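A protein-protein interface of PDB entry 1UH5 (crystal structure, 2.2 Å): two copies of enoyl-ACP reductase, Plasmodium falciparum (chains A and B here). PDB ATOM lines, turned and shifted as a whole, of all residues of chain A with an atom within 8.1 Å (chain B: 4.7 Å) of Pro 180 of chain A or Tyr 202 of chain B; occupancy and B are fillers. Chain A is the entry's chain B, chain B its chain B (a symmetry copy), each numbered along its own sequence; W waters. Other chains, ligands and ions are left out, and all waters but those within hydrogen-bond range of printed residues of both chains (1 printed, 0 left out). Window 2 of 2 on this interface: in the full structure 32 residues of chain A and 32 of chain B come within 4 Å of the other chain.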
ATOM      1  N   ASP A 130      -8.524   4.834 -21.222  1.00  0.00           N
ATOM      2  CA  ASP A 130      -7.358   4.040 -20.876  1.00  0.00           C
ATOM      3  C   ASP A 130      -6.376   4.151 -22.037  1.00  0.00           C
ATOM      4  O   ASP A 130      -6.765   4.478 -23.162  1.00  0.00           O
ATOM      5  CB  ASP A 130      -7.748   2.582 -20.618  1.00  0.00           C
ATOM      6  CG  ASP A 130      -8.431   1.947 -21.797  1.00  0.00           C
ATOM      7  OD1 ASP A 130      -7.807   1.871 -22.874  1.00  0.00           O
ATOM      8  OD2 ASP A 130      -9.592   1.524 -21.645  1.00  0.00           O
ATOM      9  N   LEU A 132      -4.868   2.087 -24.031  1.00  0.00           N
ATOM     10  CA  LEU A 132      -5.211   1.318 -25.228  1.00  0.00           C
ATOM     11  C   LEU A 132      -6.194   2.035 -26.151  1.00  0.00           C
ATOM     12  O   LEU A 132      -6.124   1.890 -27.373  1.00  0.00           O
ATOM     13  CB  LEU A 132      -5.821  -0.030 -24.835  1.00  0.00           C
ATOM     14  CG  LEU A 132      -5.259  -1.328 -25.412  1.00  0.00           C
ATOM     15  CD1 LEU A 132      -6.332  -2.396 -25.283  1.00  0.00           C
ATOM     16  CD2 LEU A 132      -4.852  -1.166 -26.869  1.00  0.00           C
ATOM     17  N   TYR A 172       4.411  11.624 -11.226  1.00  0.00           N
ATOM     18  CA  TYR A 172       3.595  10.691 -10.457  1.00  0.00           C
ATOM     19  C   TYR A 172       4.074   9.272 -10.741  1.00  0.00           C
ATOM     20  O   TYR A 172       4.511   8.966 -11.848  1.00  0.00           O
ATOM     21  CB  TYR A 172       2.114  10.859 -10.836  1.00  0.00           C
ATOM     22  CG  TYR A 172       1.154   9.972 -10.071  1.00  0.00           C
ATOM     23  CD1 TYR A 172       1.124   9.976  -8.674  1.00  0.00           C
ATOM     24  CD2 TYR A 172       0.264   9.136 -10.749  1.00  0.00           C
ATOM     25  CE1 TYR A 172       0.226   9.166  -7.969  1.00  0.00           C
ATOM     26  CE2 TYR A 172      -0.634   8.326 -10.057  1.00  0.00           C
ATOM     27  CZ  TYR A 172      -0.649   8.344  -8.670  1.00  0.00           C
ATOM     28  OH  TYR A 172      -1.535   7.540  -7.995  1.00  0.00           O
ATOM     29  N   ALA A 174       2.704   6.621 -11.478  1.00  0.00           N
ATOM     30  CA  ALA A 174       2.080   5.849 -12.560  1.00  0.00           C
ATOM     31  C   ALA A 174       3.036   5.681 -13.741  1.00  0.00           C
ATOM     32  O   ALA A 174       2.772   4.908 -14.660  1.00  0.00           O
ATOM     33  CB  ALA A 174       0.789   6.525 -13.028  1.00  0.00           C
ATOM     34  N   LYS A 177       4.910   2.309 -12.245  1.00  0.00           N
ATOM     35  CA  LYS A 177       4.036   1.187 -11.914  1.00  0.00           C
ATOM     36  C   LYS A 177       2.643   1.487 -12.436  1.00  0.00           C
ATOM     37  O   LYS A 177       2.258   2.649 -12.568  1.00  0.00           O
ATOM     38  CB  LYS A 177       4.001   0.955 -10.403  1.00  0.00           C
ATOM     39  CG  LYS A 177       5.354   0.606  -9.809  1.00  0.00           C
ATOM     40  CD  LYS A 177       5.914  -0.695 -10.383  1.00  0.00           C
ATOM     41  CE  LYS A 177       7.240  -1.051  -9.715  1.00  0.00           C
ATOM     42  NZ  LYS A 177       7.812  -2.327 -10.212  1.00  0.00           N
ATOM     43  N   VAL A 178       1.889   0.433 -12.726  1.00  0.00           N
ATOM     44  CA  VAL A 178       0.560   0.592 -13.285  1.00  0.00           C
ATOM     45  C   VAL A 178      -0.501   1.122 -12.331  1.00  0.00           C
ATOM     46  O   VAL A 178      -0.731   0.570 -11.255  1.00  0.00           O
ATOM     47  CB  VAL A 178       0.057  -0.739 -13.895  1.00  0.00           C
ATOM     48  CG1 VAL A 178      -1.341  -0.550 -14.474  1.00  0.00           C
ATOM     49  CG2 VAL A 178       1.025  -1.212 -14.972  1.00  0.00           C
ATOM     50  N   VAL A 179      -1.129   2.216 -12.744  1.00  0.00           N
ATOM     51  CA  VAL A 179      -2.207   2.826 -11.986  1.00  0.00           C
ATOM     52  C   VAL A 179      -3.388   2.922 -12.945  1.00  0.00           C
ATOM     53  O   VAL A 179      -3.430   3.793 -13.811  1.00  0.00           O
ATOM     54  CB  VAL A 179      -1.856   4.251 -11.491  1.00  0.00           C
ATOM     55  CG1 VAL A 179      -3.099   4.909 -10.878  1.00  0.00           C
ATOM     56  CG2 VAL A 179      -0.737   4.189 -10.455  1.00  0.00           C
ATOM     57  N   PRO A 180      -4.341   1.987 -12.836  1.00  0.00           N
ATOM     58  CA  PRO A 180      -5.500   2.036 -13.726  1.00  0.00           C
ATOM     59  C   PRO A 180      -6.285   3.308 -13.411  1.00  0.00           C
ATOM     60  O   PRO A 180      -6.498   3.639 -12.244  1.00  0.00           O
ATOM     61  CB  PRO A 180      -6.265   0.765 -13.361  1.00  0.00           C
ATOM     62  CG  PRO A 180      -5.175  -0.167 -12.937  1.00  0.00           C
ATOM     63  CD  PRO A 180      -4.315   0.726 -12.078  1.00  0.00           C
ATOM     64  N   GLY A 181      -6.694   4.022 -14.450  1.00  0.00           N
ATOM     65  CA  GLY A 181      -7.434   5.255 -14.246  1.00  0.00           C
ATOM     66  C   GLY A 181      -6.640   6.461 -14.708  1.00  0.00           C
ATOM     67  O   GLY A 181      -7.214   7.483 -15.080  1.00  0.00           O
ATOM     68  N   TYR A 182      -5.313   6.342 -14.680  1.00  0.00           N
ATOM     69  CA  TYR A 182      -4.418   7.419 -15.107  1.00  0.00           C
ATOM     70  C   TYR A 182      -4.240   7.255 -16.619  1.00  0.00           C
ATOM     71  O   TYR A 182      -3.201   6.768 -17.087  1.00  0.00           O
ATOM     72  CB  TYR A 182      -3.075   7.262 -14.397  1.00  0.00           C
ATOM     73  CG  TYR A 182      -2.242   8.524 -14.314  1.00  0.00           C
ATOM     74  CD1 TYR A 182      -2.680   9.622 -13.575  1.00  0.00           C
ATOM     75  CD2 TYR A 182      -0.991   8.600 -14.934  1.00  0.00           C
ATOM     76  CE1 TYR A 182      -1.894  10.762 -13.447  1.00  0.00           C
ATOM     77  CE2 TYR A 182      -0.191   9.740 -14.809  1.00  0.00           C
ATOM     78  CZ  TYR A 182      -0.649  10.813 -14.063  1.00  0.00           C
ATOM     79  OH  TYR A 182       0.141  11.925 -13.917  1.00  0.00           O
ATOM     80  N   GLY A 183      -5.249   7.667 -17.387  1.00  0.00           N
ATOM     81  CA  GLY A 183      -5.176   7.482 -18.829  1.00  0.00           C
ATOM     82  C   GLY A 183      -4.773   8.643 -19.711  1.00  0.00           C
ATOM     83  O   GLY A 183      -4.135   9.598 -19.265  1.00  0.00           O
ATOM     84  N   ILE A 228     -10.185  13.444 -13.726  1.00  0.00           N
ATOM     85  CA  ILE A 228     -10.033  12.015 -13.976  1.00  0.00           C
ATOM     86  C   ILE A 228     -11.308  11.291 -13.540  1.00  0.00           C
ATOM     87  O   ILE A 228     -11.316  10.071 -13.381  1.00  0.00           O
ATOM     88  CB  ILE A 228      -8.830  11.441 -13.188  1.00  0.00           C
ATOM     89  CG1 ILE A 228      -7.606  12.340 -13.381  1.00  0.00           C
ATOM     90  CG2 ILE A 228      -8.506  10.036 -13.672  1.00  0.00           C
ATOM     91  CD1 ILE A 228      -6.391  11.913 -12.577  1.00  0.00           C
ATOM     92  N   PHE A 273     -11.585   8.573  -8.972  1.00  0.00           N
ATOM     93  CA  PHE A 273     -10.207   8.099  -8.942  1.00  0.00           C
ATOM     94  C   PHE A 273      -9.401   8.701  -7.793  1.00  0.00           C
ATOM     95  O   PHE A 273      -8.789   7.976  -7.004  1.00  0.00           O
ATOM     96  CB  PHE A 273      -9.509   8.428 -10.264  1.00  0.00           C
ATOM     97  CG  PHE A 273      -8.013   8.331 -10.192  1.00  0.00           C
ATOM     98  CD1 PHE A 273      -7.388   7.095 -10.050  1.00  0.00           C
ATOM     99  CD2 PHE A 273      -7.230   9.481 -10.207  1.00  0.00           C
ATOM    100  CE1 PHE A 273      -6.002   7.010  -9.922  1.00  0.00           C
ATOM    101  CE2 PHE A 273      -5.844   9.405 -10.079  1.00  0.00           C
ATOM    102  CZ  PHE A 273      -5.229   8.169  -9.937  1.00  0.00           C
ATOM    103  N   TYR A 276     -10.263   7.607  -4.217  1.00  0.00           N
ATOM    104  CA  TYR A 276      -9.761   6.261  -3.987  1.00  0.00           C
ATOM    105  C   TYR A 276      -8.258   6.308  -3.695  1.00  0.00           C
ATOM    106  O   TYR A 276      -7.782   5.692  -2.739  1.00  0.00           O
ATOM    107  CB  TYR A 276     -10.027   5.387  -5.217  1.00  0.00           C
ATOM    108  CG  TYR A 276      -9.397   4.013  -5.143  1.00  0.00           C
ATOM    109  CD1 TYR A 276      -9.746   3.118  -4.133  1.00  0.00           C
ATOM    110  CD2 TYR A 276      -8.452   3.607  -6.088  1.00  0.00           C
ATOM    111  CE1 TYR A 276      -9.169   1.852  -4.063  1.00  0.00           C
ATOM    112  CE2 TYR A 276      -7.868   2.343  -6.027  1.00  0.00           C
ATOM    113  CZ  TYR A 276      -8.232   1.470  -5.012  1.00  0.00           C
ATOM    114  OH  TYR A 276      -7.664   0.217  -4.949  1.00  0.00           O
ATOM    115  N   ARG B 198       4.245  -1.592 -19.716  1.00  0.00           N
ATOM    116  CA  ARG B 198       3.666  -2.049 -18.448  1.00  0.00           C
ATOM    117  C   ARG B 198       2.148  -1.830 -18.422  1.00  0.00           C
ATOM    118  O   ARG B 198       1.394  -2.724 -18.049  1.00  0.00           O
ATOM    119  CB  ARG B 198       4.299  -1.311 -17.258  1.00  0.00           C
ATOM    120  CG  ARG B 198       5.769  -1.661 -16.999  1.00  0.00           C
ATOM    121  CD  ARG B 198       6.292  -0.965 -15.751  1.00  0.00           C
ATOM    122  NE  ARG B 198       6.596   0.453 -15.950  1.00  0.00           N
ATOM    123  CZ  ARG B 198       7.732   0.908 -16.475  1.00  0.00           C
ATOM    124  NH1 ARG B 198       8.677   0.059 -16.862  1.00  0.00           N
ATOM    125  NH2 ARG B 198       7.940   2.217 -16.581  1.00  0.00           N
ATOM    126  N   VAL B 199       1.702  -0.639 -18.812  1.00  0.00           N
ATOM    127  CA  VAL B 199       0.269  -0.342 -18.810  1.00  0.00           C
ATOM    128  C   VAL B 199      -0.475  -1.258 -19.778  1.00  0.00           C
ATOM    129  O   VAL B 199      -1.546  -1.775 -19.451  1.00  0.00           O
ATOM    130  CB  VAL B 199       0.002   1.135 -19.183  1.00  0.00           C
ATOM    131  CG1 VAL B 199      -1.504   1.434 -19.135  1.00  0.00           C
ATOM    132  CG2 VAL B 199       0.754   2.043 -18.214  1.00  0.00           C
ATOM    133  N   LEU B 200       0.091  -1.464 -20.962  1.00  0.00           N
ATOM    134  CA  LEU B 200      -0.527  -2.339 -21.951  1.00  0.00           C
ATOM    135  C   LEU B 200      -0.544  -3.784 -21.445  1.00  0.00           C
ATOM    136  O   LEU B 200      -1.462  -4.544 -21.757  1.00  0.00           O
ATOM    137  CB  LEU B 200       0.231  -2.265 -23.280  1.00  0.00           C
ATOM    138  CG  LEU B 200       0.152  -0.933 -24.042  1.00  0.00           C
ATOM    139  CD1 LEU B 200       1.063  -0.984 -25.256  1.00  0.00           C
ATOM    140  CD2 LEU B 200      -1.278  -0.665 -24.463  1.00  0.00           C
ATOM    141  N   ALA B 201       0.476  -4.165 -20.674  1.00  0.00           N
ATOM    142  CA  ALA B 201       0.540  -5.522 -20.130  1.00  0.00           C
ATOM    143  C   ALA B 201      -0.678  -5.749 -19.242  1.00  0.00           C
ATOM    144  O   ALA B 201      -1.241  -6.845 -19.211  1.00  0.00           O
ATOM    145  CB  ALA B 201       1.826  -5.724 -19.320  1.00  0.00           C
ATOM    146  N   TYR B 202      -1.079  -4.707 -18.524  1.00  0.00           N
ATOM    147  CA  TYR B 202      -2.242  -4.791 -17.646  1.00  0.00           C
ATOM    148  C   TYR B 202      -3.527  -4.977 -18.456  1.00  0.00           C
ATOM    149  O   TYR B 202      -4.265  -5.939 -18.245  1.00  0.00           O
ATOM    150  CB  TYR B 202      -2.351  -3.525 -16.794  1.00  0.00           C
ATOM    151  CG  TYR B 202      -3.657  -3.392 -16.041  1.00  0.00           C
ATOM    152  CD1 TYR B 202      -3.967  -4.238 -14.977  1.00  0.00           C
ATOM    153  CD2 TYR B 202      -4.578  -2.409 -16.387  1.00  0.00           C
ATOM    154  CE1 TYR B 202      -5.160  -4.103 -14.275  1.00  0.00           C
ATOM    155  CE2 TYR B 202      -5.772  -2.264 -15.696  1.00  0.00           C
ATOM    156  CZ  TYR B 202      -6.057  -3.112 -14.641  1.00  0.00           C
ATOM    157  OH  TYR B 202      -7.234  -2.952 -13.946  1.00  0.00           O
ATOM    158  N   HIS B 203      -3.785  -4.065 -19.389  1.00  0.00           N
ATOM    159  CA  HIS B 203      -4.989  -4.132 -20.217  1.00  0.00           C
ATOM    160  C   HIS B 203      -5.063  -5.387 -21.087  1.00  0.00           C
ATOM    161  O   HIS B 203      -6.091  -6.063 -21.122  1.00  0.00           O
ATOM    162  CB  HIS B 203      -5.093  -2.893 -21.113  1.00  0.00           C
ATOM    163  CG  HIS B 203      -5.240  -1.608 -20.355  1.00  0.00           C
ATOM    164  ND1 HIS B 203      -6.281  -1.372 -19.483  1.00  0.00           N
ATOM    165  CD2 HIS B 203      -4.474  -0.493 -20.336  1.00  0.00           C
ATOM    166  CE1 HIS B 203      -6.149  -0.166 -18.957  1.00  0.00           C
ATOM    167  NE2 HIS B 203      -5.060   0.388 -19.458  1.00  0.00           N
ATOM    168  N   LEU B 204      -3.979  -5.697 -21.793  1.00  0.00           N
ATOM    169  CA  LEU B 204      -3.953  -6.872 -22.660  1.00  0.00           C
ATOM    170  C   LEU B 204      -3.983  -8.186 -21.882  1.00  0.00           C
ATOM    171  O   LEU B 204      -4.507  -9.193 -22.362  1.00  0.00           O
ATOM    172  CB  LEU B 204      -2.715  -6.837 -23.559  1.00  0.00           C
ATOM    173  CG  LEU B 204      -2.628  -5.664 -24.542  1.00  0.00           C
ATOM    174  CD1 LEU B 204      -1.363  -5.795 -25.376  1.00  0.00           C
ATOM    175  CD2 LEU B 204      -3.851  -5.650 -25.442  1.00  0.00           C
ATOM    176  N   GLY B 205      -3.407  -8.174 -20.685  1.00  0.00           N
ATOM    177  CA  GLY B 205      -3.381  -9.375 -19.875  1.00  0.00           C
ATOM    178  C   GLY B 205      -4.746  -9.718 -19.313  1.00  0.00           C
ATOM    179  O   GLY B 205      -5.203 -10.853 -19.423  1.00  0.00           O
ATOM    180  N   ARG B 206      -5.409  -8.728 -18.727  1.00  0.00           N
ATOM    181  CA  ARG B 206      -6.723  -8.937 -18.129  1.00  0.00           C
ATOM    182  C   ARG B 206      -7.844  -9.184 -19.129  1.00  0.00           C
ATOM    183  O   ARG B 206      -8.645 -10.096 -18.950  1.00  0.00           O
ATOM    184  CB  ARG B 206      -7.107  -7.734 -17.263  1.00  0.00           C
ATOM    185  CG  ARG B 206      -6.216  -7.503 -16.053  1.00  0.00           C
ATOM    186  CD  ARG B 206      -6.254  -8.674 -15.076  1.00  0.00           C
ATOM    187  NE  ARG B 206      -5.677  -8.302 -13.786  1.00  0.00           N
ATOM    188  CZ  ARG B 206      -6.220  -7.415 -12.957  1.00  0.00           C
ATOM    189  NH1 ARG B 206      -7.359  -6.815 -13.284  1.00  0.00           N
ATOM    190  NH2 ARG B 206      -5.621  -7.110 -11.811  1.00  0.00           N
HETATM  191  O   HOH W   1       4.112   2.280 -15.854  1.00  0.00           O
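N of Leu 132 of chain A is in hydrogen-bond range of OD1 of Asp 130 of chain A, 3.2 Å away.
Asp 130 of chain A touches His 203 of chain B.
Arg 198 of chain B touches Val 178 of chain A (O to CG2, 3.4 Å).
N of Val 199 of chain B touches CG2 of Val 178 of chain A, 3.9 Å away.
Tyr 202 of chain B touches Val 178 of chain A.
Tyr 202 of chain B touches Pro 180 of chain A (CZ to CG, 3.5 Å).
Leu 132 of chain A touches none of the printed residues of chain B.
Of the printed residues of chain B, Val 178 of chain A touches Arg 198 (3.4 Å), Val 199 (3.9 Å) and Tyr 202 (3.9 Å).
Val 179 of chain A touches none of the printed residues of chain B.
Pro 180 of chain A touches just one residue of chain B: Tyr 202 (3.5 Å).
Of the printed residues of chain A, Arg 198 of chain B touches Val 178 (3.4 Å).
Of the printed residues of chain A, Val 199 of chain B touches Val 178.
Of chain A, only Val 178 (3.9 Å) and Pro 180 (3.5 Å) come within 4 Å of Tyr 202 of chain B.
The nearest residue of chain A that does not touch Tyr 202 of chain B is Val 179 of chain A (6.3 Å).
Of the 14 printed residues of chain A, 3 touch a printed residue of chain B.
Among the printed residues, 5 pairs touch across the chains.
Among the printed residues, no Asp or Glu carboxylate lies within 4 Å of a Lys or Arg side-chain nitrogen of the other chain.
No position is printed for both chains.
Water W1 lies within hydrogen-bond range of NE of Arg 198 of chain B (3.1 Å) and O of Ala 174 of chain A (3.2 Å).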
